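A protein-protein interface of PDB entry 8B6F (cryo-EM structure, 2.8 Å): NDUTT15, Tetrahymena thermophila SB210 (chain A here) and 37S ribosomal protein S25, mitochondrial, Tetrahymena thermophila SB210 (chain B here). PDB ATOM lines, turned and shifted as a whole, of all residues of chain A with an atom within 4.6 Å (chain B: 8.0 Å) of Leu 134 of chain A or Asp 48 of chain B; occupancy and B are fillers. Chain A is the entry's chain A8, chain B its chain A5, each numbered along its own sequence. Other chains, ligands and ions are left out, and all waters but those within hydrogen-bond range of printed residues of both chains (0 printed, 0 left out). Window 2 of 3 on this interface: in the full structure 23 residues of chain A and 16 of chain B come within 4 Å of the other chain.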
ATOM      1  N   ILE A 132       8.750 -27.467  21.880  1.00  0.00           N
ATOM      2  CA  ILE A 132      10.147 -27.051  21.960  1.00  0.00           C
ATOM      3  C   ILE A 132      10.765 -27.120  20.567  1.00  0.00           C
ATOM      4  O   ILE A 132      10.613 -28.138  19.878  1.00  0.00           O
ATOM      5  CB  ILE A 132      10.932 -27.917  22.959  1.00  0.00           C
ATOM      6  CG1 ILE A 132      10.292 -27.820  24.348  1.00  0.00           C
ATOM      7  CG2 ILE A 132      12.393 -27.482  23.003  1.00  0.00           C
ATOM      8  CD1 ILE A 132      10.958 -28.676  25.408  1.00  0.00           C
ATOM      9  N   PRO A 133      11.462 -26.078  20.111  1.00  0.00           N
ATOM     10  CA  PRO A 133      12.116 -26.152  18.799  1.00  0.00           C
ATOM     11  C   PRO A 133      13.113 -27.298  18.732  1.00  0.00           C
ATOM     12  O   PRO A 133      13.705 -27.697  19.736  1.00  0.00           O
ATOM     13  CB  PRO A 133      12.816 -24.795  18.675  1.00  0.00           C
ATOM     14  CG  PRO A 133      12.019 -23.889  19.531  1.00  0.00           C
ATOM     15  CD  PRO A 133      11.555 -24.725  20.687  1.00  0.00           C
ATOM     16  N   LEU A 134      13.289 -27.833  17.521  1.00  0.00           N
ATOM     17  CA  LEU A 134      14.158 -28.992  17.338  1.00  0.00           C
ATOM     18  C   LEU A 134      15.556 -28.723  17.878  1.00  0.00           C
ATOM     19  O   LEU A 134      16.101 -29.523  18.647  1.00  0.00           O
ATOM     20  CB  LEU A 134      14.217 -29.369  15.857  1.00  0.00           C
ATOM     21  CG  LEU A 134      15.119 -30.552  15.497  1.00  0.00           C
ATOM     22  CD1 LEU A 134      14.669 -31.822  16.200  1.00  0.00           C
ATOM     23  CD2 LEU A 134      15.143 -30.756  13.995  1.00  0.00           C
ATOM     24  N   ASN A 135      16.158 -27.600  17.485  1.00  0.00           N
ATOM     25  CA  ASN A 135      17.484 -27.262  17.993  1.00  0.00           C
ATOM     26  C   ASN A 135      17.453 -27.059  19.501  1.00  0.00           C
ATOM     27  O   ASN A 135      18.350 -27.517  20.216  1.00  0.00           O
ATOM     28  CB  ASN A 135      18.011 -26.012  17.295  1.00  0.00           C
ATOM     29  CG  ASN A 135      18.266 -26.233  15.820  1.00  0.00           C
ATOM     30  OD1 ASN A 135      17.844 -27.238  15.250  1.00  0.00           O
ATOM     31  ND2 ASN A 135      18.962 -25.294  15.194  1.00  0.00           N
ATOM     32  N   ASP A 136      16.430 -26.367  20.002  1.00  0.00           N
ATOM     33  CA  ASP A 136      16.299 -26.191  21.444  1.00  0.00           C
ATOM     34  C   ASP A 136      16.103 -27.528  22.144  1.00  0.00           C
ATOM     35  O   ASP A 136      16.646 -27.756  23.231  1.00  0.00           O
ATOM     36  CB  ASP A 136      15.136 -25.250  21.753  1.00  0.00           C
ATOM     37  CG  ASP A 136      15.383 -23.839  21.258  1.00  0.00           C
ATOM     38  OD1 ASP A 136      16.451 -23.597  20.659  1.00  0.00           O
ATOM     39  OD2 ASP A 136      14.509 -22.971  21.470  1.00  0.00           O
ATOM     40  N   LEU A 137      15.325 -28.427  21.537  1.00  0.00           N
ATOM     41  CA  LEU A 137      15.125 -29.746  22.129  1.00  0.00           C
ATOM     42  C   LEU A 137      16.432 -30.524  22.199  1.00  0.00           C
ATOM     43  O   LEU A 137      16.721 -31.176  23.209  1.00  0.00           O
ATOM     44  CB  LEU A 137      14.079 -30.523  21.330  1.00  0.00           C
ATOM     45  CG  LEU A 137      13.685 -31.894  21.884  1.00  0.00           C
ATOM     46  CD1 LEU A 137      13.084 -31.765  23.277  1.00  0.00           C
ATOM     47  CD2 LEU A 137      12.715 -32.590  20.947  1.00  0.00           C
ATOM     48  N   ILE A 138      17.237 -30.472  21.135  1.00  0.00           N
ATOM     49  CA  ILE A 138      18.517 -31.177  21.143  1.00  0.00           C
ATOM     50  C   ILE A 138      19.436 -30.596  22.210  1.00  0.00           C
ATOM     51  O   ILE A 138      20.110 -31.333  22.937  1.00  0.00           O
ATOM     52  CB  ILE A 138      19.161 -31.124  19.746  1.00  0.00           C
ATOM     53  CG1 ILE A 138      18.320 -31.928  18.751  1.00  0.00           C
ATOM     54  CG2 ILE A 138      20.592 -31.655  19.788  1.00  0.00           C
ATOM     55  CD1 ILE A 138      18.751 -31.773  17.309  1.00  0.00           C
ATOM     56  N   VAL A 161      11.853 -37.819  17.773  1.00  0.00           N
ATOM     57  CA  VAL A 161      11.693 -36.498  17.170  1.00  0.00           C
ATOM     58  C   VAL A 161      12.830 -36.217  16.196  1.00  0.00           C
ATOM     59  O   VAL A 161      12.613 -35.668  15.110  1.00  0.00           O
ATOM     60  CB  VAL A 161      11.599 -35.418  18.265  1.00  0.00           C
ATOM     61  CG1 VAL A 161      11.694 -34.018  17.661  1.00  0.00           C
ATOM     62  CG2 VAL A 161      10.303 -35.562  19.042  1.00  0.00           C
ATOM     63  N   HIS A 165      12.354 -35.433  12.222  1.00  0.00           N
ATOM     64  CA  HIS A 165      12.835 -34.202  11.607  1.00  0.00           C
ATOM     65  C   HIS A 165      14.269 -34.330  11.103  1.00  0.00           C
ATOM     66  O   HIS A 165      15.015 -33.346  11.097  1.00  0.00           O
ATOM     67  CB  HIS A 165      12.724 -33.039  12.593  1.00  0.00           C
ATOM     68  CG  HIS A 165      11.315 -32.682  12.947  1.00  0.00           C
ATOM     69  ND1 HIS A 165      10.613 -33.324  13.945  1.00  0.00           N
ATOM     70  CD2 HIS A 165      10.474 -31.755  12.432  1.00  0.00           C
ATOM     71  CE1 HIS A 165       9.402 -32.804  14.031  1.00  0.00           C
ATOM     72  NE2 HIS A 165       9.291 -31.851  13.123  1.00  0.00           N
ATOM     73  N   ARG A 168      15.546 -31.678   8.661  1.00  0.00           N
ATOM     74  CA  ARG A 168      15.839 -30.337   9.148  1.00  0.00           C
ATOM     75  C   ARG A 168      17.091 -30.276  10.011  1.00  0.00           C
ATOM     76  O   ARG A 168      17.423 -29.199  10.519  1.00  0.00           O
ATOM     77  CB  ARG A 168      14.647 -29.791   9.942  1.00  0.00           C
ATOM     78  CG  ARG A 168      13.367 -29.714   9.134  1.00  0.00           C
ATOM     79  CD  ARG A 168      12.447 -28.607   9.630  1.00  0.00           C
ATOM     80  NE  ARG A 168      12.001 -28.815  11.003  1.00  0.00           N
ATOM     81  CZ  ARG A 168      12.519 -28.219  12.070  1.00  0.00           C
ATOM     82  NH1 ARG A 168      13.530 -27.370  11.971  1.00  0.00           N
ATOM     83  NH2 ARG A 168      12.010 -28.482  13.269  1.00  0.00           N
ATOM     84  N   LEU A 169      17.786 -31.393  10.199  1.00  0.00           N
ATOM     85  CA  LEU A 169      18.962 -31.406  11.056  1.00  0.00           C
ATOM     86  C   LEU A 169      20.093 -30.588  10.446  1.00  0.00           C
ATOM     87  O   LEU A 169      20.362 -30.660   9.245  1.00  0.00           O
ATOM     88  CB  LEU A 169      19.428 -32.840  11.295  1.00  0.00           C
ATOM     89  CG  LEU A 169      18.516 -33.719  12.152  1.00  0.00           C
ATOM     90  CD1 LEU A 169      19.059 -35.136  12.218  1.00  0.00           C
ATOM     91  CD2 LEU A 169      18.353 -33.147  13.552  1.00  0.00           C
ATOM     92  N   GLU B  43      21.035 -16.461  11.971  1.00  0.00           N
ATOM     93  CA  GLU B  43      20.418 -17.276  13.014  1.00  0.00           C
ATOM     94  C   GLU B  43      19.612 -16.422  13.982  1.00  0.00           C
ATOM     95  O   GLU B  43      18.520 -16.817  14.406  1.00  0.00           O
ATOM     96  CB  GLU B  43      21.487 -18.069  13.766  1.00  0.00           C
ATOM     97  CG  GLU B  43      22.133 -19.180  12.950  1.00  0.00           C
ATOM     98  CD  GLU B  43      23.102 -18.662  11.907  1.00  0.00           C
ATOM     99  OE1 GLU B  43      23.359 -17.441  11.883  1.00  0.00           O
ATOM    100  OE2 GLU B  43      23.608 -19.478  11.108  1.00  0.00           O
ATOM    101  N   HIS B  45      17.971 -13.738  13.496  1.00  0.00           N
ATOM    102  CA  HIS B  45      16.711 -13.328  12.896  1.00  0.00           C
ATOM    103  C   HIS B  45      15.828 -14.497  12.479  1.00  0.00           C
ATOM    104  O   HIS B  45      14.644 -14.286  12.198  1.00  0.00           O
ATOM    105  CB  HIS B  45      16.975 -12.438  11.676  1.00  0.00           C
ATOM    106  CG  HIS B  45      17.759 -11.203  11.993  1.00  0.00           C
ATOM    107  ND1 HIS B  45      19.118 -11.108  11.783  1.00  0.00           N
ATOM    108  CD2 HIS B  45      17.375 -10.014  12.515  1.00  0.00           C
ATOM    109  CE1 HIS B  45      19.536  -9.913  12.156  1.00  0.00           C
ATOM    110  NE2 HIS B  45      18.499  -9.229  12.606  1.00  0.00           N
ATOM    111  N   GLN B  46      16.364 -15.715  12.432  1.00  0.00           N
ATOM    112  CA  GLN B  46      15.547 -16.869  12.077  1.00  0.00           C
ATOM    113  C   GLN B  46      14.475 -17.110  13.131  1.00  0.00           C
ATOM    114  O   GLN B  46      14.693 -16.902  14.328  1.00  0.00           O
ATOM    115  CB  GLN B  46      16.421 -18.112  11.922  1.00  0.00           C
ATOM    116  CG  GLN B  46      17.140 -18.196  10.585  1.00  0.00           C
ATOM    117  CD  GLN B  46      18.067 -19.390  10.499  1.00  0.00           C
ATOM    118  OE1 GLN B  46      17.991 -20.308  11.313  1.00  0.00           O
ATOM    119  NE2 GLN B  46      18.958 -19.377   9.515  1.00  0.00           N
ATOM    120  N   ILE B  47      13.304 -17.553  12.677  1.00  0.00           N
ATOM    121  CA  ILE B  47      12.168 -17.849  13.542  1.00  0.00           C
ATOM    122  C   ILE B  47      11.696 -19.261  13.231  1.00  0.00           C
ATOM    123  O   ILE B  47      11.568 -19.632  12.059  1.00  0.00           O
ATOM    124  CB  ILE B  47      11.019 -16.841  13.349  1.00  0.00           C
ATOM    125  CG1 ILE B  47      11.525 -15.411  13.561  1.00  0.00           C
ATOM    126  CG2 ILE B  47       9.876 -17.155  14.308  1.00  0.00           C
ATOM    127  CD1 ILE B  47      10.494 -14.337  13.277  1.00  0.00           C
ATOM    128  N   ASP B  48      11.440 -20.043  14.273  1.00  0.00           N
ATOM    129  CA  ASP B  48      10.951 -21.404  14.125  1.00  0.00           C
ATOM    130  C   ASP B  48       9.435 -21.436  14.275  1.00  0.00           C
ATOM    131  O   ASP B  48       8.849 -20.646  15.018  1.00  0.00           O
ATOM    132  CB  ASP B  48      11.596 -22.332  15.156  1.00  0.00           C
ATOM    133  CG  ASP B  48      11.264 -23.790  14.913  1.00  0.00           C
ATOM    134  OD1 ASP B  48      10.538 -24.080  13.941  1.00  0.00           O
ATOM    135  OD2 ASP B  48      11.731 -24.648  15.688  1.00  0.00           O
ATOM    136  N   TYR B  49       8.804 -22.372  13.565  1.00  0.00           N
ATOM    137  CA  TYR B  49       7.348 -22.457  13.560  1.00  0.00           C
ATOM    138  C   TYR B  49       6.774 -22.870  14.908  1.00  0.00           C
ATOM    139  O   TYR B  49       5.561 -22.742  15.106  1.00  0.00           O
ATOM    140  CB  TYR B  49       6.883 -23.434  12.481  1.00  0.00           C
ATOM    141  CG  TYR B  49       7.257 -24.872  12.741  1.00  0.00           C
ATOM    142  CD1 TYR B  49       6.411 -25.713  13.451  1.00  0.00           C
ATOM    143  CD2 TYR B  49       8.450 -25.396  12.262  1.00  0.00           C
ATOM    144  CE1 TYR B  49       6.744 -27.029  13.683  1.00  0.00           C
ATOM    145  CE2 TYR B  49       8.793 -26.711  12.488  1.00  0.00           C
ATOM    146  CZ  TYR B  49       7.936 -27.524  13.200  1.00  0.00           C
ATOM    147  OH  TYR B  49       8.274 -28.836  13.429  1.00  0.00           O
ATOM    148  N   LYS B  50       7.599 -23.357  15.829  1.00  0.00           N
ATOM    149  CA  LYS B  50       7.143 -23.717  17.163  1.00  0.00           C
ATOM    150  C   LYS B  50       7.194 -22.546  18.134  1.00  0.00           C
ATOM    151  O   LYS B  50       6.895 -22.729  19.317  1.00  0.00           O
ATOM    152  CB  LYS B  50       7.977 -24.879  17.714  1.00  0.00           C
ATOM    153  CG  LYS B  50       7.708 -26.207  17.025  1.00  0.00           C
ATOM    154  CD  LYS B  50       8.491 -27.335  17.675  1.00  0.00           C
ATOM    155  CE  LYS B  50       8.187 -28.673  17.023  1.00  0.00           C
ATOM    156  NZ  LYS B  50       6.757 -29.059  17.164  1.00  0.00           N
ATOM    157  N   THR B  51       7.568 -21.358  17.665  1.00  0.00           N
ATOM    158  CA  THR B  51       7.595 -20.190  18.532  1.00  0.00           C
ATOM    159  C   THR B  51       6.212 -19.938  19.118  1.00  0.00           C
ATOM    160  O   THR B  51       5.197 -20.026  18.422  1.00  0.00           O
ATOM    161  CB  THR B  51       8.066 -18.961  17.752  1.00  0.00           C
ATOM    162  OG1 THR B  51       9.323 -19.240  17.123  1.00  0.00           O
ATOM    163  CG2 THR B  51       8.228 -17.765  18.678  1.00  0.00           C
ATOM    164  N   ALA B  52       6.180 -19.620  20.409  1.00  0.00           N
ATOM    165  CA  ALA B  52       4.916 -19.404  21.094  1.00  0.00           C
ATOM    166  C   ALA B  52       4.203 -18.185  20.524  1.00  0.00           C
ATOM    167  O   ALA B  52       4.828 -17.247  20.026  1.00  0.00           O
ATOM    168  CB  ALA B  52       5.150 -19.222  22.593  1.00  0.00           C
ATOM    169  N   SER B  56       5.523 -14.807  19.028  1.00  0.00           N
ATOM    170  CA  SER B  56       5.566 -14.887  17.577  1.00  0.00           C
ATOM    171  C   SER B  56       5.282 -13.533  16.948  1.00  0.00           C
ATOM    172  O   SER B  56       4.795 -12.612  17.606  1.00  0.00           O
ATOM    173  CB  SER B  56       4.525 -15.883  17.087  1.00  0.00           C
ATOM    174  OG  SER B  56       3.239 -15.358  17.359  1.00  0.00           O
ATOM    175  N   PRO B  57       5.582 -13.374  15.655  1.00  0.00           N
ATOM    176  CA  PRO B  57       5.220 -12.129  14.961  1.00  0.00           C
ATOM    177  C   PRO B  57       3.723 -11.942  14.774  1.00  0.00           C
ATOM    178  O   PRO B  57       3.312 -10.916  14.219  1.00  0.00           O
ATOM    179  CB  PRO B  57       5.920 -12.268  13.597  1.00  0.00           C
ATOM    180  CG  PRO B  57       6.877 -13.401  13.737  1.00  0.00           C
ATOM    181  CD  PRO B  57       6.310 -14.302  14.775  1.00  0.00           C
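The backbone carbonyl oxygen (O) of Val 161 of chain A lies within hydrogen-bond range of a ring nitrogen (ND1) of His 165 of chain A (3.3 Å). OG1 of Thr 51 of chain B is in hydrogen-bond range of O of Asp 48 of chain B (2.6 Å).
The side-chain hydroxyl (OH) of Tyr 49 of chain B sits at hydrogen-bond distance from a ring nitrogen (NE2) of His 165 of chain A.
CD of Lys 50 of chain B touches O of Ile 132 of chain A, 3.2 Å away. OD2 of Asp 48 of chain B touches CB of Pro 133 of chain A, at 3.2 Å. CA of Pro 133 of chain A touches CD of Lys 50 of chain B (3.98 Å). Leu 134 of chain A touches Asp 48 of chain B (N to OD2, 3.99 Å). NH2 of Arg 168 of chain A touches CE2 of Tyr 49 of chain B (3.8 Å).
Printed residues of chain B within 4 Å of Ile 132 of chain A: Lys 50 (3.2 Å). Of the printed residues of chain B, Pro 133 of chain A touches Asp 48 (3.2 Å) and Lys 50 (3.98 Å). Of the printed residues of chain B, Leu 134 of chain A touches Asp 48. Printed residues of chain B within 4 Å of His 165 of chain A: Tyr 49. Of the printed residues of chain A, Asp 48 of chain B touches Pro 133 (3.2 Å) and Leu 134 (3.99 Å). Of the printed residues of chain A, Tyr 49 of chain B touches His 165 and Arg 168. Printed residues of chain A within 4 Å of Lys 50 of chain B: Ile 132 (3.2 Å) and Pro 133 (3.98 Å). The nearest printed residue of chain B that does not touch Leu 134 of chain A is Lys 50 of chain B (4.8 Å). The nearest printed residue of chain A that does not touch Asp 48 of chain B is Arg 168 of chain A (4.5 Å).
Of the 11 printed residues of chain A, 5 touch a printed residue of chain B. Hydrophobic or aromatic side chains of chain A within 4 Å of the printed part of chain B: Pro 133 and His 165. Of the 11 printed residues of chain B, 3 touch a printed residue of chain A. Among the printed residues, 6 pairs touch across the chains. Among the printed residues, no Asp or Glu carboxylate lies within 4 Å of a Lys or Arg side-chain nitrogen of the other chain.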
